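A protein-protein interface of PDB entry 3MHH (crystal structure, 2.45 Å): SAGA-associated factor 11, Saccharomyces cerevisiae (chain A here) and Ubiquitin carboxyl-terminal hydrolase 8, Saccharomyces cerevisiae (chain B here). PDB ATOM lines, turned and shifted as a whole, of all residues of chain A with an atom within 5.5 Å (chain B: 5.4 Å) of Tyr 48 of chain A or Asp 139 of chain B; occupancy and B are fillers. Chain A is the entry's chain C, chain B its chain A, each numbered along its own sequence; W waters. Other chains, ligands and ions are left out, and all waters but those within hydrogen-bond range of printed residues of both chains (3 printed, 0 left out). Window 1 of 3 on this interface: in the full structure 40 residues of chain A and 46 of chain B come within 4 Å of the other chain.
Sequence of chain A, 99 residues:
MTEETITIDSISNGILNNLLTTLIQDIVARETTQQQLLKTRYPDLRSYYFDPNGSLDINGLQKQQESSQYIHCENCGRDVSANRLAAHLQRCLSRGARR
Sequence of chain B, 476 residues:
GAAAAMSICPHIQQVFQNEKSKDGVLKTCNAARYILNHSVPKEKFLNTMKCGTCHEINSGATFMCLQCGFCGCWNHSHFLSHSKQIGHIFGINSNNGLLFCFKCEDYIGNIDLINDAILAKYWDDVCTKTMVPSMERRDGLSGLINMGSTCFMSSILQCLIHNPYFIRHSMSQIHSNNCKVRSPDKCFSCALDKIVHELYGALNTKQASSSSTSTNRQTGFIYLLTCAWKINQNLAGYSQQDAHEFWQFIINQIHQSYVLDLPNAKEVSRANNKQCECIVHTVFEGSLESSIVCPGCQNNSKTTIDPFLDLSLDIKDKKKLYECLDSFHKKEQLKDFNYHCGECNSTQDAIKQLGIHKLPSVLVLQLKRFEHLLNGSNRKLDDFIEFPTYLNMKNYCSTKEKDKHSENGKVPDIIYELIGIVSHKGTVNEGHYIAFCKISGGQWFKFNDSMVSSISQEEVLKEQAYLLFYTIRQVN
OE1 of Glu 136 of chain B is in salt-bridge range of NH2 of Arg 46 of chain A (3.3 Å).
The side-chain hydroxyl (OH) of Tyr 48 of chain A sits close to the side-chain carboxylate (OD2) of Asp 139 of chain B (2.4 Å).
O of Tyr 49 of chain A sits at hydrogen-bond distance from OG of Ser 454 of chain B, 3.0 Å away.
O of Met 135 of chain B sits at hydrogen-bond distance from NH1 of Arg 138 of chain B (2.9 Å).
O of Leu 141 of chain B sits at hydrogen-bond distance from NH1 of Arg 137 of chain B.
The backbone NH (N) of Tyr 49 of chain A sits at hydrogen-bond distance from the backbone carbonyl oxygen (O) of Ile 58 of chain A.
The side-chain carboxylate of Asp 139 of chain B lies within salt-bridge range of the guanidinium group of Arg 138 of chain B, 3.6 Å away.
Among the printed residues, merely in contact across the chains: Arg 46 of chain A with Met 135 of chain B, Tyr 48 of chain A with Arg 138 of chain B, Tyr 48 of chain A with Leu 141 of chain B, Tyr 48 of chain A with Phe 445 of chain B, Phe 50 of chain A with Ser 454 of chain B, Ile 58 of chain A with Leu 141 of chain B, Ile 58 of chain A with Phe 445 of chain B and Ile 58 of chain A with Ser 454 of chain B.
Of chain B, only Arg 138, Asp 139, Leu 141 and Phe 445 come within 4 Å of Tyr 48 of chain A.
Of chain A, only Tyr 48 (2.4 Å) comes within 4 Å of Asp 139 of chain B.
Printed residues of chain A within 4 Å of Leu 141 of chain B: Tyr 48 and Ile 58.
Printed residues of chain A within 4 Å of Phe 445 of chain B: Tyr 48 (3.5 Å) and Ile 58 (3.7 Å).
The nearest printed residue of chain B that does not touch Phe 50 of chain A is Phe 445 of chain B (8.2 Å).
Hydrophobic or aromatic side chains of chain A that line the printed part of chain B: Tyr 48, Phe 50 and Ile 58.
Of the 13 printed residues of chain B, 7 touch a printed residue of chain A.
Hydrophobic or aromatic side chains of chain B that line the printed part of chain A: Met 135, Leu 141 and Phe 445.
Among the printed residues, Asp or Glu carboxylates within 4 Å of a Lys or Arg side-chain nitrogen of the other chain: Arg 46 of chain A with Glu 136 of chain B.
Water W3 lies within hydrogen-bond range of O of Arg 46 of chain A, NH2 of Arg 138 of chain B and N of Tyr 48 of chain A.
Water W1 lies within hydrogen-bond range of O of Tyr 49 of chain A and N of Ser 454 of chain B.
Water W2 lies within hydrogen-bond range of the guanidinium group of Arg 138 of chain B and the backbone carbonyl oxygen of Arg 46 of chain A.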
ATOM      1  N   ARG A  46     -12.636 -14.240  24.866  1.00  0.00           N
ATOM      2  CA  ARG A  46     -13.411 -13.585  23.829  1.00  0.00           C
ATOM      3  C   ARG A  46     -12.526 -13.436  22.593  1.00  0.00           C
ATOM      4  O   ARG A  46     -11.328 -13.182  22.699  1.00  0.00           O
ATOM      5  CB  ARG A  46     -13.904 -12.221  24.331  1.00  0.00           C
ATOM      6  CG  ARG A  46     -13.066 -11.641  25.470  1.00  0.00           C
ATOM      7  CD  ARG A  46     -13.675 -10.371  26.063  1.00  0.00           C
ATOM      8  NE  ARG A  46     -12.827  -9.789  27.106  1.00  0.00           N
ATOM      9  CZ  ARG A  46     -11.710  -9.099  26.869  1.00  0.00           C
ATOM     10  NH1 ARG A  46     -11.299  -8.903  25.623  1.00  0.00           N
ATOM     11  NH2 ARG A  46     -10.998  -8.603  27.875  1.00  0.00           N
ATOM     12  N   SER A  47     -13.104 -13.638  21.418  1.00  0.00           N
ATOM     13  CA  SER A  47     -12.365 -13.460  20.178  1.00  0.00           C
ATOM     14  C   SER A  47     -12.047 -11.979  19.986  1.00  0.00           C
ATOM     15  O   SER A  47     -12.674 -11.117  20.597  1.00  0.00           O
ATOM     16  CB  SER A  47     -13.196 -13.931  18.992  1.00  0.00           C
ATOM     17  OG  SER A  47     -13.660 -12.808  18.261  1.00  0.00           O
ATOM     18  N   TYR A  48     -11.074 -11.675  19.137  1.00  0.00           N
ATOM     19  CA  TYR A  48     -10.779 -10.284  18.848  1.00  0.00           C
ATOM     20  C   TYR A  48     -11.902  -9.803  17.948  1.00  0.00           C
ATOM     21  O   TYR A  48     -12.383 -10.558  17.105  1.00  0.00           O
ATOM     22  CB  TYR A  48      -9.411 -10.129  18.183  1.00  0.00           C
ATOM     23  CG  TYR A  48      -8.247 -10.609  19.030  1.00  0.00           C
ATOM     24  CD1 TYR A  48      -7.899  -9.975  20.224  1.00  0.00           C
ATOM     25  CD2 TYR A  48      -7.487 -11.690  18.631  1.00  0.00           C
ATOM     26  CE1 TYR A  48      -6.810 -10.427  20.999  1.00  0.00           C
ATOM     27  CE2 TYR A  48      -6.419 -12.160  19.400  1.00  0.00           C
ATOM     28  CZ  TYR A  48      -6.078 -11.526  20.570  1.00  0.00           C
ATOM     29  OH  TYR A  48      -4.995 -12.005  21.289  1.00  0.00           O
ATOM     30  N   TYR A  49     -12.370  -8.582  18.171  1.00  0.00           N
ATOM     31  CA  TYR A  49     -13.427  -8.005  17.345  1.00  0.00           C
ATOM     32  C   TYR A  49     -12.966  -7.806  15.896  1.00  0.00           C
ATOM     33  O   TYR A  49     -11.828  -7.390  15.652  1.00  0.00           O
ATOM     34  CB  TYR A  49     -13.845  -6.657  17.918  1.00  0.00           C
ATOM     35  CG  TYR A  49     -15.115  -6.099  17.332  1.00  0.00           C
ATOM     36  CD1 TYR A  49     -16.330  -6.288  17.969  1.00  0.00           C
ATOM     37  CD2 TYR A  49     -15.101  -5.350  16.165  1.00  0.00           C
ATOM     38  CE1 TYR A  49     -17.507  -5.766  17.453  1.00  0.00           C
ATOM     39  CE2 TYR A  49     -16.275  -4.826  15.639  1.00  0.00           C
ATOM     40  CZ  TYR A  49     -17.482  -5.038  16.294  1.00  0.00           C
ATOM     41  OH  TYR A  49     -18.676  -4.528  15.789  1.00  0.00           O
ATOM     42  N   PHE A  50     -13.864  -8.086  14.950  1.00  0.00           N
ATOM     43  CA  PHE A  50     -13.603  -7.838  13.543  1.00  0.00           C
ATOM     44  C   PHE A  50     -14.677  -6.967  12.929  1.00  0.00           C
ATOM     45  O   PHE A  50     -15.859  -7.279  13.002  1.00  0.00           O
ATOM     46  CB  PHE A  50     -13.529  -9.132  12.754  1.00  0.00           C
ATOM     47  CG  PHE A  50     -13.458  -8.917  11.276  1.00  0.00           C
ATOM     48  CD1 PHE A  50     -12.239  -8.736  10.647  1.00  0.00           C
ATOM     49  CD2 PHE A  50     -14.617  -8.857  10.514  1.00  0.00           C
ATOM     50  CE1 PHE A  50     -12.173  -8.522   9.284  1.00  0.00           C
ATOM     51  CE2 PHE A  50     -14.557  -8.644   9.144  1.00  0.00           C
ATOM     52  CZ  PHE A  50     -13.333  -8.479   8.530  1.00  0.00           C
ATOM     53  N   ILE A  58      -9.544  -4.328  18.001  1.00  0.00           N
ATOM     54  CA  ILE A  58      -9.725  -5.689  18.477  1.00  0.00           C
ATOM     55  C   ILE A  58     -10.530  -5.788  19.778  1.00  0.00           C
ATOM     56  O   ILE A  58     -10.828  -6.893  20.247  1.00  0.00           O
ATOM     57  CB  ILE A  58      -8.380  -6.403  18.630  1.00  0.00           C
ATOM     58  CG1 ILE A  58      -7.446  -5.609  19.546  1.00  0.00           C
ATOM     59  CG2 ILE A  58      -7.739  -6.618  17.252  1.00  0.00           C
ATOM     60  CD1 ILE A  58      -6.175  -6.343  19.884  1.00  0.00           C
ATOM     61  N   MET B 135      -4.858 -12.962  29.486  1.00  0.00           N
ATOM     62  CA  MET B 135      -5.635 -13.043  28.259  1.00  0.00           C
ATOM     63  C   MET B 135      -5.299 -11.892  27.310  1.00  0.00           C
ATOM     64  O   MET B 135      -5.116 -12.100  26.107  1.00  0.00           O
ATOM     65  CB  MET B 135      -7.124 -12.991  28.618  1.00  0.00           C
ATOM     66  CG  MET B 135      -8.030 -13.604  27.591  1.00  0.00           C
ATOM     67  SD  MET B 135      -9.769 -13.359  27.980  1.00  0.00           S
ATOM     68  CE  MET B 135      -9.994 -11.693  27.376  1.00  0.00           C
ATOM     69  N   GLU B 136      -5.203 -10.684  27.860  1.00  0.00           N
ATOM     70  CA  GLU B 136      -5.041  -9.482  27.054  1.00  0.00           C
ATOM     71  C   GLU B 136      -3.653  -9.300  26.434  1.00  0.00           C
ATOM     72  O   GLU B 136      -3.514  -8.637  25.404  1.00  0.00           O
ATOM     73  CB  GLU B 136      -5.379  -8.245  27.876  1.00  0.00           C
ATOM     74  CG  GLU B 136      -6.854  -8.107  28.215  1.00  0.00           C
ATOM     75  CD  GLU B 136      -7.214  -8.759  29.527  1.00  0.00           C
ATOM     76  OE1 GLU B 136      -8.382  -8.591  29.960  1.00  0.00           O
ATOM     77  OE2 GLU B 136      -6.335  -9.434  30.122  1.00  0.00           O
ATOM     78  N   ARG B 137      -2.631  -9.886  27.049  1.00  0.00           N
ATOM     79  CA  ARG B 137      -1.255  -9.658  26.604  1.00  0.00           C
ATOM     80  C   ARG B 137      -0.681 -10.869  25.884  1.00  0.00           C
ATOM     81  O   ARG B 137       0.419 -10.801  25.345  1.00  0.00           O
ATOM     82  CB  ARG B 137      -0.367  -9.346  27.809  1.00  0.00           C
ATOM     83  CG  ARG B 137      -0.842  -8.200  28.673  1.00  0.00           C
ATOM     84  CD  ARG B 137      -0.583  -6.830  28.026  1.00  0.00           C
ATOM     85  NE  ARG B 137      -1.781  -6.285  27.387  1.00  0.00           N
ATOM     86  CZ  ARG B 137      -1.926  -6.088  26.077  1.00  0.00           C
ATOM     87  NH1 ARG B 137      -0.932  -6.361  25.228  1.00  0.00           N
ATOM     88  NH2 ARG B 137      -3.060  -5.566  25.616  1.00  0.00           N
ATOM     89  N   ARG B 138      -1.415 -11.979  25.898  1.00  0.00           N
ATOM     90  CA  ARG B 138      -0.871 -13.255  25.433  1.00  0.00           C
ATOM     91  C   ARG B 138      -0.309 -13.199  24.015  1.00  0.00           C
ATOM     92  O   ARG B 138       0.616 -13.944  23.687  1.00  0.00           O
ATOM     93  CB  ARG B 138      -1.918 -14.362  25.537  1.00  0.00           C
ATOM     94  CG  ARG B 138      -2.987 -14.295  24.460  1.00  0.00           C
ATOM     95  CD  ARG B 138      -4.131 -15.256  24.746  1.00  0.00           C
ATOM     96  NE  ARG B 138      -4.979 -15.434  23.574  1.00  0.00           N
ATOM     97  CZ  ARG B 138      -6.028 -14.677  23.290  1.00  0.00           C
ATOM     98  NH1 ARG B 138      -6.388 -13.690  24.099  1.00  0.00           N
ATOM     99  NH2 ARG B 138      -6.736 -14.920  22.201  1.00  0.00           N
ATOM    100  N   ASP B 139      -0.857 -12.323  23.173  1.00  0.00           N
ATOM    101  CA  ASP B 139      -0.408 -12.242  21.787  1.00  0.00           C
ATOM    102  C   ASP B 139       0.421 -11.003  21.512  1.00  0.00           C
ATOM    103  O   ASP B 139       0.732 -10.700  20.369  1.00  0.00           O
ATOM    104  CB  ASP B 139      -1.605 -12.303  20.844  1.00  0.00           C
ATOM    105  CG  ASP B 139      -2.264 -13.671  20.835  1.00  0.00           C
ATOM    106  OD1 ASP B 139      -1.534 -14.663  20.976  1.00  0.00           O
ATOM    107  OD2 ASP B 139      -3.509 -13.753  20.721  1.00  0.00           O
ATOM    108  N   GLY B 140       0.788 -10.288  22.562  1.00  0.00           N
ATOM    109  CA  GLY B 140       1.625  -9.101  22.425  1.00  0.00           C
ATOM    110  C   GLY B 140       1.011  -7.908  21.719  1.00  0.00           C
ATOM    111  O   GLY B 140       1.714  -6.969  21.392  1.00  0.00           O
ATOM    112  N   LEU B 141      -0.303  -7.912  21.522  1.00  0.00           N
ATOM    113  CA  LEU B 141      -0.955  -6.888  20.714  1.00  0.00           C
ATOM    114  C   LEU B 141      -1.225  -5.619  21.496  1.00  0.00           C
ATOM    115  O   LEU B 141      -1.920  -5.640  22.525  1.00  0.00           O
ATOM    116  CB  LEU B 141      -2.269  -7.408  20.144  1.00  0.00           C
ATOM    117  CG  LEU B 141      -2.150  -8.637  19.255  1.00  0.00           C
ATOM    118  CD1 LEU B 141      -3.529  -9.159  18.891  1.00  0.00           C
ATOM    119  CD2 LEU B 141      -1.340  -8.293  18.016  1.00  0.00           C
ATOM    120  N   HIS B 162       6.654  -8.881  16.734  1.00  0.00           N
ATOM    121  CA  HIS B 162       5.987 -10.124  16.302  1.00  0.00           C
ATOM    122  C   HIS B 162       6.875 -11.000  15.406  1.00  0.00           C
ATOM    123  O   HIS B 162       6.394 -11.779  14.607  1.00  0.00           O
ATOM    124  CB  HIS B 162       4.645  -9.813  15.620  1.00  0.00           C
ATOM    125  CG  HIS B 162       3.673  -9.128  16.528  1.00  0.00           C
ATOM    126  ND1 HIS B 162       2.938  -9.806  17.475  1.00  0.00           N
ATOM    127  CD2 HIS B 162       3.363  -7.817  16.676  1.00  0.00           C
ATOM    128  CE1 HIS B 162       2.186  -8.946  18.139  1.00  0.00           C
ATOM    129  NE2 HIS B 162       2.445  -7.729  17.693  1.00  0.00           N
ATOM    130  N   LEU B 199       4.239  -5.450  26.456  1.00  0.00           N
ATOM    131  CA  LEU B 199       3.269  -5.961  25.513  1.00  0.00           C
ATOM    132  C   LEU B 199       2.837  -7.388  25.822  1.00  0.00           C
ATOM    133  O   LEU B 199       1.707  -7.752  25.539  1.00  0.00           O
ATOM    134  CB  LEU B 199       3.818  -5.872  24.085  1.00  0.00           C
ATOM    135  CG  LEU B 199       3.562  -4.556  23.336  1.00  0.00           C
ATOM    136  CD1 LEU B 199       4.049  -3.371  24.112  1.00  0.00           C
ATOM    137  CD2 LEU B 199       4.223  -4.588  21.959  1.00  0.00           C
ATOM    138  N   TYR B 200       3.732  -8.178  26.412  1.00  0.00           N
ATOM    139  CA  TYR B 200       3.490  -9.603  26.661  1.00  0.00           C
ATOM    140  C   TYR B 200       3.353  -9.956  28.149  1.00  0.00           C
ATOM    141  O   TYR B 200       2.780 -10.993  28.507  1.00  0.00           O
ATOM    142  CB  TYR B 200       4.636 -10.415  26.066  1.00  0.00           C
ATOM    143  CG  TYR B 200       4.587 -10.554  24.562  1.00  0.00           C
ATOM    144  CD1 TYR B 200       3.816 -11.543  23.965  1.00  0.00           C
ATOM    145  CD2 TYR B 200       5.330  -9.723  23.743  1.00  0.00           C
ATOM    146  CE1 TYR B 200       3.787 -11.708  22.603  1.00  0.00           C
ATOM    147  CE2 TYR B 200       5.306  -9.874  22.382  1.00  0.00           C
ATOM    148  CZ  TYR B 200       4.537 -10.877  21.810  1.00  0.00           C
ATOM    149  OH  TYR B 200       4.500 -11.028  20.436  1.00  0.00           O
ATOM    150  N   ILE B 439       0.263 -13.709  13.181  1.00  0.00           N
ATOM    151  CA  ILE B 439       0.642 -14.442  14.376  1.00  0.00           C
ATOM    152  C   ILE B 439       0.064 -15.834  14.245  1.00  0.00           C
ATOM    153  O   ILE B 439      -0.573 -16.147  13.245  1.00  0.00           O
ATOM    154  CB  ILE B 439       0.096 -13.766  15.670  1.00  0.00           C
ATOM    155  CG1 ILE B 439      -1.402 -14.022  15.845  1.00  0.00           C
ATOM    156  CG2 ILE B 439       0.374 -12.257  15.652  1.00  0.00           C
ATOM    157  CD1 ILE B 439      -2.005 -13.249  17.020  1.00  0.00           C
ATOM    158  N   PHE B 445      -3.045  -8.887  11.714  1.00  0.00           N
ATOM    159  CA  PHE B 445      -3.412  -7.687  12.451  1.00  0.00           C
ATOM    160  C   PHE B 445      -2.775  -6.444  11.854  1.00  0.00           C
ATOM    161  O   PHE B 445      -1.608  -6.443  11.493  1.00  0.00           O
ATOM    162  CB  PHE B 445      -3.030  -7.827  13.920  1.00  0.00           C
ATOM    163  CG  PHE B 445      -3.848  -8.843  14.649  1.00  0.00           C
ATOM    164  CD1 PHE B 445      -5.083  -8.496  15.196  1.00  0.00           C
ATOM    165  CD2 PHE B 445      -3.407 -10.154  14.763  1.00  0.00           C
ATOM    166  CE1 PHE B 445      -5.834  -9.418  15.846  1.00  0.00           C
ATOM    167  CE2 PHE B 445      -4.163 -11.083  15.413  1.00  0.00           C
ATOM    168  CZ  PHE B 445      -5.387 -10.713  15.962  1.00  0.00           C
ATOM    169  N   SER B 454      -8.138  -6.263  13.476  1.00  0.00           N
ATOM    170  CA  SER B 454      -7.978  -7.507  12.724  1.00  0.00           C
ATOM    171  C   SER B 454      -8.371  -7.220  11.293  1.00  0.00           C
ATOM    172  O   SER B 454      -9.162  -6.314  11.026  1.00  0.00           O
ATOM    173  CB  SER B 454      -8.843  -8.630  13.296  1.00  0.00           C
ATOM    174  OG  SER B 454     -10.194  -8.245  13.289  1.00  0.00           O
HETATM  175  O   HOH W   1     -10.634  -4.913  14.655  1.00  0.00           O
HETATM  176  O   HOH W   2      -8.659 -11.613  24.084  1.00  0.00           O
HETATM  177  O   HOH W   3      -9.223 -13.319  21.283  1.00  0.00           O
